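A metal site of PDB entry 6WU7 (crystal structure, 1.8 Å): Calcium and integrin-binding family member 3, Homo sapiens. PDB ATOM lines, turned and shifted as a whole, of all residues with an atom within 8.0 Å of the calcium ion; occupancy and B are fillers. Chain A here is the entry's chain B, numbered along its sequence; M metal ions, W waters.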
ATOM      1  N   GLU A  18       1.145  -9.021   9.687  1.00  0.00           N
ATOM      2  CA  GLU A  18      -0.221  -8.811  10.152  1.00  0.00           C
ATOM      3  C   GLU A  18      -0.398  -9.326  11.583  1.00  0.00           C
ATOM      4  O   GLU A  18      -0.977  -8.633  12.424  1.00  0.00           O
ATOM      5  CB  GLU A  18      -1.224  -9.503   9.224  1.00  0.00           C
ATOM      6  CG  GLU A  18      -1.414  -8.803   7.888  1.00  0.00           C
ATOM      7  CD  GLU A  18      -1.938  -7.389   8.053  1.00  0.00           C
ATOM      8  OE1 GLU A  18      -2.972  -7.197   8.725  1.00  0.00           O
ATOM      9  OE2 GLU A  18      -1.307  -6.451   7.498  1.00  0.00           O
ATOM     10  N   ALA A  19       0.087 -10.542  11.871  1.00  0.00           N
ATOM     11  CA  ALA A  19      -0.052 -11.080  13.222  1.00  0.00           C
ATOM     12  C   ALA A  19       0.674 -10.230  14.262  1.00  0.00           C
ATOM     13  O   ALA A  19       0.193 -10.111  15.409  1.00  0.00           O
ATOM     14  CB  ALA A  19       0.463 -12.512  13.298  1.00  0.00           C
ATOM     15  N   TYR A  20       1.815  -9.637  13.902  1.00  0.00           N
ATOM     16  CA  TYR A  20       2.522  -8.795  14.866  1.00  0.00           C
ATOM     17  C   TYR A  20       1.795  -7.475  15.084  1.00  0.00           C
ATOM     18  O   TYR A  20       1.715  -6.977  16.215  1.00  0.00           O
ATOM     19  CB  TYR A  20       3.952  -8.499  14.411  1.00  0.00           C
ATOM     20  CG  TYR A  20       4.968  -9.603  14.622  1.00  0.00           C
ATOM     21  CD1 TYR A  20       5.091 -10.245  15.855  1.00  0.00           C
ATOM     22  CD2 TYR A  20       5.809  -9.994  13.581  1.00  0.00           C
ATOM     23  CE1 TYR A  20       6.019 -11.239  16.036  1.00  0.00           C
ATOM     24  CE2 TYR A  20       6.750 -10.993  13.758  1.00  0.00           C
ATOM     25  CZ  TYR A  20       6.847 -11.610  14.980  1.00  0.00           C
ATOM     26  OH  TYR A  20       7.782 -12.598  15.151  1.00  0.00           O
ATOM     27  N   GLN A  21       1.301  -6.888  14.000  1.00  0.00           N
ATOM     28  CA  GLN A  21       0.521  -5.660  14.128  1.00  0.00           C
ATOM     29  C   GLN A  21      -0.698  -5.905  14.976  1.00  0.00           C
ATOM     30  O   GLN A  21      -1.059  -5.058  15.791  1.00  0.00           O
ATOM     31  CB  GLN A  21       0.114  -5.135  12.745  1.00  0.00           C
ATOM     32  CG  GLN A  21      -0.749  -3.875  12.773  1.00  0.00           C
ATOM     33  CD  GLN A  21      -0.863  -3.223  11.410  1.00  0.00           C
ATOM     34  OE1 GLN A  21      -0.229  -2.195  11.137  1.00  0.00           O
ATOM     35  NE2 GLN A  21      -1.650  -3.821  10.540  1.00  0.00           N
ATOM     36  N   ASP A  22      -1.343  -7.073  14.797  1.00  0.00           N
ATOM     37  CA  ASP A  22      -2.492  -7.453  15.617  1.00  0.00           C
ATOM     38  C   ASP A  22      -2.106  -7.491  17.087  1.00  0.00           C
ATOM     39  O   ASP A  22      -2.708  -6.815  17.925  1.00  0.00           O
ATOM     40  CB  ASP A  22      -3.032  -8.851  15.206  1.00  0.00           C
ATOM     41  CG  ASP A  22      -3.838  -8.862  13.896  1.00  0.00           C
ATOM     42  OD1 ASP A  22      -4.216  -7.808  13.385  1.00  0.00           O
ATOM     43  OD2 ASP A  22      -4.100  -9.980  13.362  1.00  0.00           O
ATOM     44  N   CYS A  23      -1.139  -8.331  17.444  1.00  0.00           N
ATOM     45  CA  CYS A  23      -0.986  -8.665  18.853  1.00  0.00           C
ATOM     46  C   CYS A  23      -0.258  -7.583  19.639  1.00  0.00           C
ATOM     47  O   CYS A  23      -0.551  -7.403  20.822  1.00  0.00           O
ATOM     48  CB  CYS A  23      -0.306 -10.016  19.040  1.00  0.00           C
ATOM     49  SG  CYS A  23       1.378 -10.106  18.455  1.00  0.00           S
ATOM     50  N   THR A  24       0.652  -6.847  19.005  1.00  0.00           N
ATOM     51  CA  THR A  24       1.326  -5.729  19.657  1.00  0.00           C
ATOM     52  C   THR A  24       0.554  -4.439  19.442  1.00  0.00           C
ATOM     53  O   THR A  24      -0.440  -4.399  18.721  1.00  0.00           O
ATOM     54  CB  THR A  24       2.753  -5.545  19.120  1.00  0.00           C
ATOM     55  OG1 THR A  24       2.667  -4.985  17.798  1.00  0.00           O
ATOM     56  CG2 THR A  24       3.512  -6.856  19.089  1.00  0.00           C
ATOM     57  N   PHE A  25       1.030  -3.344  20.037  1.00  0.00           N
ATOM     58  CA  PHE A  25       0.452  -2.035  19.797  1.00  0.00           C
ATOM     59  C   PHE A  25       1.144  -1.310  18.653  1.00  0.00           C
ATOM     60  O   PHE A  25       0.909  -0.114  18.465  1.00  0.00           O
ATOM     61  CB  PHE A  25       0.515  -1.184  21.065  1.00  0.00           C
ATOM     62  CG  PHE A  25      -0.328  -1.738  22.183  1.00  0.00           C
ATOM     63  CD1 PHE A  25      -1.697  -1.656  22.112  1.00  0.00           C
ATOM     64  CD2 PHE A  25       0.256  -2.373  23.258  1.00  0.00           C
ATOM     65  CE1 PHE A  25      -2.479  -2.177  23.114  1.00  0.00           C
ATOM     66  CE2 PHE A  25      -0.532  -2.900  24.271  1.00  0.00           C
ATOM     67  CZ  PHE A  25      -1.882  -2.816  24.184  1.00  0.00           C
ATOM     68  N   PHE A  26       1.967  -1.998  17.886  1.00  0.00           N
ATOM     69  CA  PHE A  26       2.737  -1.359  16.839  1.00  0.00           C
ATOM     70  C   PHE A  26       2.085  -1.554  15.478  1.00  0.00           C
ATOM     71  O   PHE A  26       1.320  -2.498  15.265  1.00  0.00           O
ATOM     72  CB  PHE A  26       4.169  -1.944  16.803  1.00  0.00           C
ATOM     73  CG  PHE A  26       4.944  -1.744  18.076  1.00  0.00           C
ATOM     74  CD1 PHE A  26       5.217  -0.474  18.549  1.00  0.00           C
ATOM     75  CD2 PHE A  26       5.398  -2.828  18.788  1.00  0.00           C
ATOM     76  CE1 PHE A  26       5.912  -0.289  19.709  1.00  0.00           C
ATOM     77  CE2 PHE A  26       6.106  -2.663  19.963  1.00  0.00           C
ATOM     78  CZ  PHE A  26       6.346  -1.397  20.435  1.00  0.00           C
ATOM     79  N   THR A  27       2.440  -0.666  14.547  1.00  0.00           N
ATOM     80  CA  THR A  27       2.142  -0.848  13.130  1.00  0.00           C
ATOM     81  C   THR A  27       3.147  -1.800  12.489  1.00  0.00           C
ATOM     82  O   THR A  27       4.207  -2.090  13.053  1.00  0.00           O
ATOM     83  CB  THR A  27       2.206   0.487  12.392  1.00  0.00           C
ATOM     84  OG1 THR A  27       3.552   0.991  12.459  1.00  0.00           O
ATOM     85  CG2 THR A  27       1.268   1.501  12.977  1.00  0.00           C
ATOM     86  N   SER A 100       6.261  -3.421  23.294  1.00  0.00           N
ATOM     87  CA  SER A 100       4.834  -3.127  23.199  1.00  0.00           C
ATOM     88  C   SER A 100       4.266  -2.705  24.553  1.00  0.00           C
ATOM     89  O   SER A 100       3.526  -1.728  24.666  1.00  0.00           O
ATOM     90  CB  SER A 100       4.103  -4.355  22.663  1.00  0.00           C
ATOM     91  OG  SER A 100       2.766  -4.032  22.324  1.00  0.00           O
HETATM   92 CA    CA M   1      -2.455  -4.261  17.503  1.00  0.00          CA
HETATM   93  O   HOH W   1      -3.165  -2.248  18.220  1.00  0.00           O
HETATM   94  O   HOH W   2      -4.824  -4.916  17.481  1.00  0.00           O
HETATM   95  O   HOH W   3      -3.124  -4.455  19.892  1.00  0.00           O
HETATM   96  O   HOH W   4      -3.863  -3.670  15.443  1.00  0.00           O
HETATM   97  O   HOH W   5      -1.161  -2.269  16.441  1.00  0.00           O
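Water W1 is bound to the calcium ion, at 2.3 Å. The backbone carbonyl oxygen (O) of Gln 21 is bound to the calcium ion (2.3 Å). O of Thr 24 binds the calcium ion (2.4 Å). Water W2 binds the calcium ion (2.5 Å). The calcium ion is bound by water W3, at 2.5 Å. Water W4 is bound to the calcium ion, at 2.6 Å. The calcium ion is bound by the backbone carbonyl oxygen (O) of Asp 22 (2.6 Å). Water W5 is bound to the calcium ion, at 2.6 Å. The calcium ion has eight donor atoms within binding distance.
Of the 11 residues printed, 3 come within 4 Å of the calcium ion. The nearest printed residue that does not touch the calcium ion is Cys 23 (4.3 Å).
The backbone NH (N) of Phe 26 sits at hydrogen-bond distance from the side-chain hydroxyl (OG1) of Thr 24, 3.1 Å away. The side-chain hydroxyl of Thr 24 sits at hydrogen-bond distance from the backbone carbonyl oxygen of Tyr 20 (2.7 Å).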
